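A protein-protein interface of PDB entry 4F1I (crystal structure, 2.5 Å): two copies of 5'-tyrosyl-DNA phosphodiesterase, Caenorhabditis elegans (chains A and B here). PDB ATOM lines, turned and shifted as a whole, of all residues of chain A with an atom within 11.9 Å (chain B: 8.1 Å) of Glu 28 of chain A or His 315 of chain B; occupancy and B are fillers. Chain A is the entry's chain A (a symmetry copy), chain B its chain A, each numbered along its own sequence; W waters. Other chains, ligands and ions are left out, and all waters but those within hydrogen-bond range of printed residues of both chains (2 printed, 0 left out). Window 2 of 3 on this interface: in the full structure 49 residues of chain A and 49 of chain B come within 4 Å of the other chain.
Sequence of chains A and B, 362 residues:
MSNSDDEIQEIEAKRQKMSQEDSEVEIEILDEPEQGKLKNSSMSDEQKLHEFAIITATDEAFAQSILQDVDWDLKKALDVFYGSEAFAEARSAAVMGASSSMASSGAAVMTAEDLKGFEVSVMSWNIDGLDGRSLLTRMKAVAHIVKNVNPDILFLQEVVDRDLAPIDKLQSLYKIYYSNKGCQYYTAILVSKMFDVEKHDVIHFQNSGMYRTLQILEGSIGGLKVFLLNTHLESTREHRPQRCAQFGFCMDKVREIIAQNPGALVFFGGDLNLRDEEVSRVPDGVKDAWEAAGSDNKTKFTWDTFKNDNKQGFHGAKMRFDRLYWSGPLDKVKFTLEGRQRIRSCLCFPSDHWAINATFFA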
ATOM      1  N   GLU A  24       5.183  -4.965 -23.064  1.00  0.00           N
ATOM      2  CA  GLU A  24       4.421  -3.982 -23.817  1.00  0.00           C
ATOM      3  C   GLU A  24       2.985  -4.472 -24.011  1.00  0.00           C
ATOM      4  O   GLU A  24       2.727  -5.676 -24.031  1.00  0.00           O
ATOM      5  CB  GLU A  24       5.092  -3.699 -25.161  1.00  0.00           C
ATOM      6  CG  GLU A  24       5.333  -4.936 -25.999  1.00  0.00           C
ATOM      7  CD  GLU A  24       6.109  -4.642 -27.269  1.00  0.00           C
ATOM      8  OE1 GLU A  24       7.021  -3.787 -27.233  1.00  0.00           O
ATOM      9  OE2 GLU A  24       5.800  -5.261 -28.309  1.00  0.00           O
ATOM     10  N   VAL A  25       2.052  -3.534 -24.124  1.00  0.00           N
ATOM     11  CA  VAL A  25       0.660  -3.880 -24.365  1.00  0.00           C
ATOM     12  C   VAL A  25       0.197  -3.289 -25.690  1.00  0.00           C
ATOM     13  O   VAL A  25       0.292  -2.081 -25.908  1.00  0.00           O
ATOM     14  CB  VAL A  25      -0.254  -3.386 -23.230  1.00  0.00           C
ATOM     15  CG1 VAL A  25      -1.680  -3.865 -23.461  1.00  0.00           C
ATOM     16  CG2 VAL A  25       0.266  -3.877 -21.886  1.00  0.00           C
ATOM     17  N   GLU A  26      -0.305  -4.152 -26.568  1.00  0.00           N
ATOM     18  CA  GLU A  26      -0.633  -3.766 -27.938  1.00  0.00           C
ATOM     19  C   GLU A  26      -1.967  -3.032 -28.070  1.00  0.00           C
ATOM     20  O   GLU A  26      -2.922  -3.312 -27.343  1.00  0.00           O
ATOM     21  CB  GLU A  26      -0.599  -4.998 -28.856  1.00  0.00           C
ATOM     22  CG  GLU A  26      -0.806  -4.694 -30.335  1.00  0.00           C
ATOM     23  CD  GLU A  26       0.240  -3.745 -30.895  1.00  0.00           C
ATOM     24  OE1 GLU A  26       1.381  -4.194 -31.137  1.00  0.00           O
ATOM     25  OE2 GLU A  26      -0.080  -2.553 -31.092  1.00  0.00           O
ATOM     26  N   ILE A  27      -2.015  -2.089 -29.004  1.00  0.00           N
ATOM     27  CA  ILE A  27      -3.238  -1.364 -29.337  1.00  0.00           C
ATOM     28  C   ILE A  27      -4.321  -2.297 -29.887  1.00  0.00           C
ATOM     29  O   ILE A  27      -4.043  -3.178 -30.703  1.00  0.00           O
ATOM     30  CB  ILE A  27      -2.954  -0.247 -30.370  1.00  0.00           C
ATOM     31  CG1 ILE A  27      -2.137   0.883 -29.737  1.00  0.00           C
ATOM     32  CG2 ILE A  27      -4.246   0.306 -30.952  1.00  0.00           C
ATOM     33  CD1 ILE A  27      -0.635   0.718 -29.878  1.00  0.00           C
ATOM     34  N   GLU A  28      -5.553  -2.105 -29.423  1.00  0.00           N
ATOM     35  CA  GLU A  28      -6.695  -2.871 -29.907  1.00  0.00           C
ATOM     36  C   GLU A  28      -7.238  -2.307 -31.212  1.00  0.00           C
ATOM     37  O   GLU A  28      -7.578  -1.128 -31.288  1.00  0.00           O
ATOM     38  CB  GLU A  28      -7.818  -2.861 -28.873  1.00  0.00           C
ATOM     39  CG  GLU A  28      -7.772  -3.981 -27.862  1.00  0.00           C
ATOM     40  CD  GLU A  28      -9.050  -4.062 -27.047  1.00  0.00           C
ATOM     41  OE1 GLU A  28      -9.630  -2.997 -26.742  1.00  0.00           O
ATOM     42  OE2 GLU A  28      -9.482  -5.190 -26.723  1.00  0.00           O
ATOM     43  N   ILE A  29      -7.313  -3.147 -32.239  1.00  0.00           N
ATOM     44  CA  ILE A  29      -8.046  -2.802 -33.452  1.00  0.00           C
ATOM     45  C   ILE A  29      -9.410  -3.482 -33.384  1.00  0.00           C
ATOM     46  O   ILE A  29      -9.507  -4.705 -33.488  1.00  0.00           O
ATOM     47  CB  ILE A  29      -7.324  -3.282 -34.724  1.00  0.00           C
ATOM     48  CG1 ILE A  29      -5.821  -3.004 -34.645  1.00  0.00           C
ATOM     49  CG2 ILE A  29      -7.938  -2.629 -35.955  1.00  0.00           C
ATOM     50  CD1 ILE A  29      -5.457  -1.557 -34.850  1.00  0.00           C
ATOM     51  N   LEU A  30     -10.460  -2.689 -33.208  1.00  0.00           N
ATOM     52  CA  LEU A  30     -11.789  -3.221 -32.914  1.00  0.00           C
ATOM     53  C   LEU A  30     -12.367  -4.153 -33.988  1.00  0.00           C
ATOM     54  O   LEU A  30     -13.026  -5.140 -33.662  1.00  0.00           O
ATOM     55  CB  LEU A  30     -12.764  -2.081 -32.607  1.00  0.00           C
ATOM     56  CG  LEU A  30     -13.964  -2.459 -31.738  1.00  0.00           C
ATOM     57  CD1 LEU A  30     -13.513  -3.231 -30.511  1.00  0.00           C
ATOM     58  CD2 LEU A  30     -14.733  -1.220 -31.330  1.00  0.00           C
ATOM     59  N   ASP A  31     -12.111  -3.853 -35.258  1.00  0.00           N
ATOM     60  CA  ASP A  31     -12.661  -4.653 -36.344  1.00  0.00           C
ATOM     61  C   ASP A  31     -11.647  -5.650 -36.904  1.00  0.00           C
ATOM     62  O   ASP A  31     -11.731  -6.066 -38.060  1.00  0.00           O
ATOM     63  CB  ASP A  31     -13.209  -3.753 -37.455  1.00  0.00           C
ATOM     64  CG  ASP A  31     -12.126  -2.955 -38.152  1.00  0.00           C
ATOM     65  OD1 ASP A  31     -11.143  -2.563 -37.484  1.00  0.00           O
ATOM     66  OD2 ASP A  31     -12.260  -2.723 -39.374  1.00  0.00           O
ATOM     67  N   GLU A  32     -10.693  -6.036 -36.065  1.00  0.00           N
ATOM     68  CA  GLU A  32      -9.672  -7.002 -36.448  1.00  0.00           C
ATOM     69  C   GLU A  32     -10.085  -8.398 -35.987  1.00  0.00           C
ATOM     70  O   GLU A  32     -10.734  -8.536 -34.949  1.00  0.00           O
ATOM     71  CB  GLU A  32      -8.343  -6.601 -35.807  1.00  0.00           C
ATOM     72  CG  GLU A  32      -7.129  -7.378 -36.274  1.00  0.00           C
ATOM     73  CD  GLU A  32      -5.855  -6.902 -35.609  1.00  0.00           C
ATOM     74  OE1 GLU A  32      -4.769  -7.099 -36.191  1.00  0.00           O
ATOM     75  OE2 GLU A  32      -5.942  -6.328 -34.501  1.00  0.00           O
ATOM     76  N   PRO A  33      -9.739  -9.436 -36.769  1.00  0.00           N
ATOM     77  CA  PRO A  33      -9.932 -10.818 -36.321  1.00  0.00           C
ATOM     78  C   PRO A  33      -9.304 -11.032 -34.946  1.00  0.00           C
ATOM     79  O   PRO A  33      -8.141 -10.682 -34.740  1.00  0.00           O
ATOM     80  CB  PRO A  33      -9.191 -11.629 -37.382  1.00  0.00           C
ATOM     81  CG  PRO A  33      -9.330 -10.815 -38.614  1.00  0.00           C
ATOM     82  CD  PRO A  33      -9.283  -9.373 -38.168  1.00  0.00           C
ATOM     83  N   GLU A  34     -10.074 -11.596 -34.022  1.00  0.00           N
ATOM     84  CA  GLU A  34      -9.691 -11.632 -32.615  1.00  0.00           C
ATOM     85  C   GLU A  34      -8.887 -12.864 -32.228  1.00  0.00           C
ATOM     86  O   GLU A  34      -9.050 -13.398 -31.133  1.00  0.00           O
ATOM     87  CB  GLU A  34     -10.930 -11.534 -31.721  1.00  0.00           C
ATOM     88  CG  GLU A  34     -12.033 -12.502 -32.098  1.00  0.00           C
ATOM     89  CD  GLU A  34     -13.069 -11.874 -33.007  1.00  0.00           C
ATOM     90  OE1 GLU A  34     -12.899 -11.926 -34.246  1.00  0.00           O
ATOM     91  OE2 GLU A  34     -14.055 -11.326 -32.476  1.00  0.00           O
ATOM     92  N   GLN A  35      -8.019 -13.307 -33.130  1.00  0.00           N
ATOM     93  CA  GLN A  35      -7.113 -14.410 -32.842  1.00  0.00           C
ATOM     94  C   GLN A  35      -5.984 -14.446 -33.857  1.00  0.00           C
ATOM     95  O   GLN A  35      -6.222 -14.592 -35.057  1.00  0.00           O
ATOM     96  CB  GLN A  35      -7.852 -15.750 -32.856  1.00  0.00           C
ATOM     97  CG  GLN A  35      -8.131 -16.336 -31.479  1.00  0.00           C
ATOM     98  CD  GLN A  35      -8.726 -17.731 -31.550  1.00  0.00           C
ATOM     99  OE1 GLN A  35      -8.219 -18.601 -32.262  1.00  0.00           O
ATOM    100  NE2 GLN A  35      -9.814 -17.951 -30.816  1.00  0.00           N
ATOM    101  N   ARG B 237       0.662  -1.004 -36.029  1.00  0.00           N
ATOM    102  CA  ARG B 237       1.130  -2.382 -36.118  1.00  0.00           C
ATOM    103  C   ARG B 237       1.036  -2.935 -37.537  1.00  0.00           C
ATOM    104  O   ARG B 237       1.948  -3.619 -37.999  1.00  0.00           O
ATOM    105  CB  ARG B 237       0.348  -3.281 -35.156  1.00  0.00           C
ATOM    106  CG  ARG B 237       0.972  -4.654 -34.967  1.00  0.00           C
ATOM    107  CD  ARG B 237       0.267  -5.458 -33.892  1.00  0.00           C
ATOM    108  NE  ARG B 237      -0.519  -6.556 -34.447  1.00  0.00           N
ATOM    109  CZ  ARG B 237      -1.834  -6.518 -34.637  1.00  0.00           C
ATOM    110  NH1 ARG B 237      -2.526  -5.432 -34.316  1.00  0.00           N
ATOM    111  NH2 ARG B 237      -2.458  -7.570 -35.147  1.00  0.00           N
ATOM    112  N   TRP B 303       5.327   5.686 -24.662  1.00  0.00           N
ATOM    113  CA  TRP B 303       3.966   5.956 -25.103  1.00  0.00           C
ATOM    114  C   TRP B 303       3.044   5.092 -24.254  1.00  0.00           C
ATOM    115  O   TRP B 303       2.846   3.916 -24.543  1.00  0.00           O
ATOM    116  CB  TRP B 303       3.815   5.618 -26.586  1.00  0.00           C
ATOM    117  CG  TRP B 303       2.560   6.140 -27.218  1.00  0.00           C
ATOM    118  CD1 TRP B 303       2.337   7.410 -27.662  1.00  0.00           C
ATOM    119  CD2 TRP B 303       1.367   5.401 -27.502  1.00  0.00           C
ATOM    120  NE1 TRP B 303       1.075   7.512 -28.196  1.00  0.00           N
ATOM    121  CE2 TRP B 303       0.458   6.291 -28.109  1.00  0.00           C
ATOM    122  CE3 TRP B 303       0.976   4.074 -27.297  1.00  0.00           C
ATOM    123  CZ2 TRP B 303      -0.819   5.899 -28.513  1.00  0.00           C
ATOM    124  CZ3 TRP B 303      -0.287   3.685 -27.701  1.00  0.00           C
ATOM    125  CH2 TRP B 303      -1.171   4.595 -28.300  1.00  0.00           C
ATOM    126  N   THR B 305      -0.630   4.748 -22.526  1.00  0.00           N
ATOM    127  CA  THR B 305      -2.031   5.156 -22.452  1.00  0.00           C
ATOM    128  C   THR B 305      -2.626   4.996 -21.043  1.00  0.00           C
ATOM    129  O   THR B 305      -3.579   5.689 -20.674  1.00  0.00           O
ATOM    130  CB  THR B 305      -2.847   4.430 -23.551  1.00  0.00           C
ATOM    131  OG1 THR B 305      -2.852   5.247 -24.727  1.00  0.00           O
ATOM    132  CG2 THR B 305      -4.275   4.148 -23.126  1.00  0.00           C
ATOM    133  N   PHE B 306      -2.031   4.113 -20.244  1.00  0.00           N
ATOM    134  CA  PHE B 306      -2.409   3.973 -18.841  1.00  0.00           C
ATOM    135  C   PHE B 306      -2.062   5.231 -18.051  1.00  0.00           C
ATOM    136  O   PHE B 306      -2.747   5.579 -17.090  1.00  0.00           O
ATOM    137  CB  PHE B 306      -1.683   2.796 -18.196  1.00  0.00           C
ATOM    138  CG  PHE B 306      -2.007   1.464 -18.802  1.00  0.00           C
ATOM    139  CD1 PHE B 306      -1.210   0.934 -19.800  1.00  0.00           C
ATOM    140  CD2 PHE B 306      -3.095   0.731 -18.357  1.00  0.00           C
ATOM    141  CE1 PHE B 306      -1.494  -0.299 -20.353  1.00  0.00           C
ATOM    142  CE2 PHE B 306      -3.387  -0.504 -18.903  1.00  0.00           C
ATOM    143  CZ  PHE B 306      -2.586  -1.019 -19.903  1.00  0.00           C
ATOM    144  N   LYS B 311      -4.603  10.654 -25.051  1.00  0.00           N
ATOM    145  CA  LYS B 311      -5.392   9.750 -25.868  1.00  0.00           C
ATOM    146  C   LYS B 311      -5.984   8.659 -24.999  1.00  0.00           C
ATOM    147  O   LYS B 311      -5.334   8.164 -24.080  1.00  0.00           O
ATOM    148  CB  LYS B 311      -4.546   9.147 -26.983  1.00  0.00           C
ATOM    149  CG  LYS B 311      -4.188  10.149 -28.052  1.00  0.00           C
ATOM    150  CD  LYS B 311      -3.352   9.523 -29.138  1.00  0.00           C
ATOM    151  CE  LYS B 311      -2.847  10.585 -30.088  1.00  0.00           C
ATOM    152  NZ  LYS B 311      -2.004  10.021 -31.185  1.00  0.00           N
ATOM    153  N   GLN B 312      -7.227   8.296 -25.292  1.00  0.00           N
ATOM    154  CA  GLN B 312      -7.956   7.339 -24.476  1.00  0.00           C
ATOM    155  C   GLN B 312      -8.513   6.210 -25.324  1.00  0.00           C
ATOM    156  O   GLN B 312      -9.115   6.437 -26.374  1.00  0.00           O
ATOM    157  CB  GLN B 312      -9.100   8.035 -23.740  1.00  0.00           C
ATOM    158  CG  GLN B 312      -8.683   9.287 -22.996  1.00  0.00           C
ATOM    159  CD  GLN B 312      -9.747  10.366 -23.037  1.00  0.00           C
ATOM    160  OE1 GLN B 312      -9.615  11.357 -23.756  1.00  0.00           O
ATOM    161  NE2 GLN B 312     -10.812  10.176 -22.266  1.00  0.00           N
ATOM    162  N   GLY B 313      -8.298   4.987 -24.858  1.00  0.00           N
ATOM    163  CA  GLY B 313      -8.889   3.816 -25.471  1.00  0.00           C
ATOM    164  C   GLY B 313      -9.719   3.113 -24.422  1.00  0.00           C
ATOM    165  O   GLY B 313      -9.687   3.491 -23.254  1.00  0.00           O
ATOM    166  N   PHE B 314     -10.474   2.102 -24.831  1.00  0.00           N
ATOM    167  CA  PHE B 314     -11.214   1.298 -23.874  1.00  0.00           C
ATOM    168  C   PHE B 314     -10.225   0.559 -22.984  1.00  0.00           C
ATOM    169  O   PHE B 314     -10.438   0.416 -21.784  1.00  0.00           O
ATOM    170  CB  PHE B 314     -12.113   0.302 -24.600  1.00  0.00           C
ATOM    171  CG  PHE B 314     -12.993  -0.496 -23.687  1.00  0.00           C
ATOM    172  CD1 PHE B 314     -14.065   0.100 -23.046  1.00  0.00           C
ATOM    173  CD2 PHE B 314     -12.757  -1.844 -23.478  1.00  0.00           C
ATOM    174  CE1 PHE B 314     -14.884  -0.633 -22.209  1.00  0.00           C
ATOM    175  CE2 PHE B 314     -13.573  -2.583 -22.642  1.00  0.00           C
ATOM    176  CZ  PHE B 314     -14.638  -1.976 -22.008  1.00  0.00           C
ATOM    177  N   HIS B 315      -9.139   0.095 -23.592  1.00  0.00           N
ATOM    178  CA  HIS B 315      -8.069  -0.563 -22.861  1.00  0.00           C
ATOM    179  C   HIS B 315      -6.790   0.249 -22.954  1.00  0.00           C
ATOM    180  O   HIS B 315      -6.531   0.912 -23.960  1.00  0.00           O
ATOM    181  CB  HIS B 315      -7.823  -1.967 -23.410  1.00  0.00           C
ATOM    182  CG  HIS B 315      -8.899  -2.940 -23.054  1.00  0.00           C
ATOM    183  ND1 HIS B 315      -9.205  -4.036 -23.836  1.00  0.00           N
ATOM    184  CD2 HIS B 315      -9.751  -2.980 -22.003  1.00  0.00           C
ATOM    185  CE1 HIS B 315     -10.196  -4.707 -23.277  1.00  0.00           C
ATOM    186  NE2 HIS B 315     -10.545  -4.088 -22.164  1.00  0.00           N
ATOM    187  N   GLY B 316      -5.995   0.197 -21.893  1.00  0.00           N
ATOM    188  CA  GLY B 316      -4.699   0.837 -21.899  1.00  0.00           C
ATOM    189  C   GLY B 316      -3.759   0.173 -22.886  1.00  0.00           C
ATOM    190  O   GLY B 316      -3.931  -0.992 -23.245  1.00  0.00           O
ATOM    191  N   ALA B 317      -2.762   0.926 -23.331  1.00  0.00           N
ATOM    192  CA  ALA B 317      -1.724   0.398 -24.201  1.00  0.00           C
ATOM    193  C   ALA B 317      -0.404   1.062 -23.832  1.00  0.00           C
ATOM    194  O   ALA B 317      -0.385   2.214 -23.402  1.00  0.00           O
ATOM    195  CB  ALA B 317      -2.067   0.665 -25.658  1.00  0.00           C
ATOM    196  N   LYS B 318       0.700   0.338 -23.978  1.00  0.00           N
ATOM    197  CA  LYS B 318       2.007   0.923 -23.700  1.00  0.00           C
ATOM    198  C   LYS B 318       3.119   0.285 -24.519  1.00  0.00           C
ATOM    199  O   LYS B 318       3.147  -0.929 -24.716  1.00  0.00           O
ATOM    200  CB  LYS B 318       2.329   0.904 -22.202  1.00  0.00           C
ATOM    201  CG  LYS B 318       2.365  -0.463 -21.565  1.00  0.00           C
ATOM    202  CD  LYS B 318       2.608  -0.328 -20.072  1.00  0.00           C
ATOM    203  CE  LYS B 318       2.740  -1.678 -19.399  1.00  0.00           C
ATOM    204  NZ  LYS B 318       2.938  -1.520 -17.932  1.00  0.00           N
HETATM  205  O   HOH W   1      -4.963  -2.116 -25.565  1.00  0.00           O
HETATM  206  O   HOH W   2      -5.921  -0.376 -27.119  1.00  0.00           O
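NH2 of Arg 237 of chain B lies within salt-bridge range of OE1 of Glu 32 of chain A.
ND1 of His 315 of chain B sits at hydrogen-bond distance from OE1 of Glu 28 of chain A (3.1 Å).
The backbone carbonyl oxygen (O) of Lys 318 of chain B lies within hydrogen-bond range of the backbone NH (N) of Val 25 of chain A (2.9 Å).
N of Thr 305 of chain B is in hydrogen-bond range of O of Ala 317 of chain B (2.7 Å).
O of Lys 318 of chain B touches CB of Glu 24 of chain A (3.4 Å).
CG1 of Val 25 of chain A touches O of Gly 316 of chain B, 3.7 Å away.
Val 25 of chain A touches Ala 317 of chain B (O to CA, 3.6 Å).
OE1 of Glu 26 of chain A touches CD of Arg 237 of chain B (3.2 Å).
Trp 303 of chain B touches Ile 27 of chain A.
Printed residues of chain B within 4 Å of Glu 24 of chain A: Lys 318.
Of the printed residues of chain B, Val 25 of chain A touches Gly 316, Ala 317 and Lys 318.
Of chain B, only His 315 (3.1 Å) comes within 4 Å of Glu 28 of chain A.
Ile 29 of chain A touches none of the printed residues of chain B.
Of the printed residues of chain B, Glu 32 of chain A touches Arg 237 (2.6 Å).
Pro 33 of chain A touches none of the printed residues of chain B.
Of the printed residues of chain A, Trp 303 of chain B touches Ile 27.
No residue of chain A comes within 4 Å of Thr 305 of chain B.
No residue of chain A comes within 4 Å of Gly 313 of chain B.
No residue of chain A comes within 4 Å of Phe 314 of chain B.
Ala 317 of chain B touches just one residue of chain A: Val 25 (3.6 Å).
Of the printed residues of chain A, Lys 318 of chain B touches Glu 24 and Val 25.
The nearest residue of chain B that does not touch Glu 28 of chain A is Phe 314 of chain B (4.7 Å).
The nearest printed residue of chain B that does not touch Val 25 of chain A is Phe 306 of chain B (4.3 Å).
Hydrophobic or aromatic side chains of chain B that line the printed part of chain A: Trp 303, His 315 and Ala 317.
Hydrophobic or aromatic side chains of chain A that line the printed part of chain B: Val 25 and Ile 27.
Among the printed residues, Asp or Glu carboxylates within 4 Å of a Lys or Arg side-chain nitrogen of the other chain: Glu 32 of chain A with Arg 237 of chain B.
No position is printed for both chains.
Water W1 bridges O of Gly 316 of chain B (2.8 Å) and O of Glu 26 of chain A (3.0 Å).
Water W2 bridges the backbone NH (N) of Glu 28 of chain A and the backbone carbonyl oxygen (O) of His 315 of chain B.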
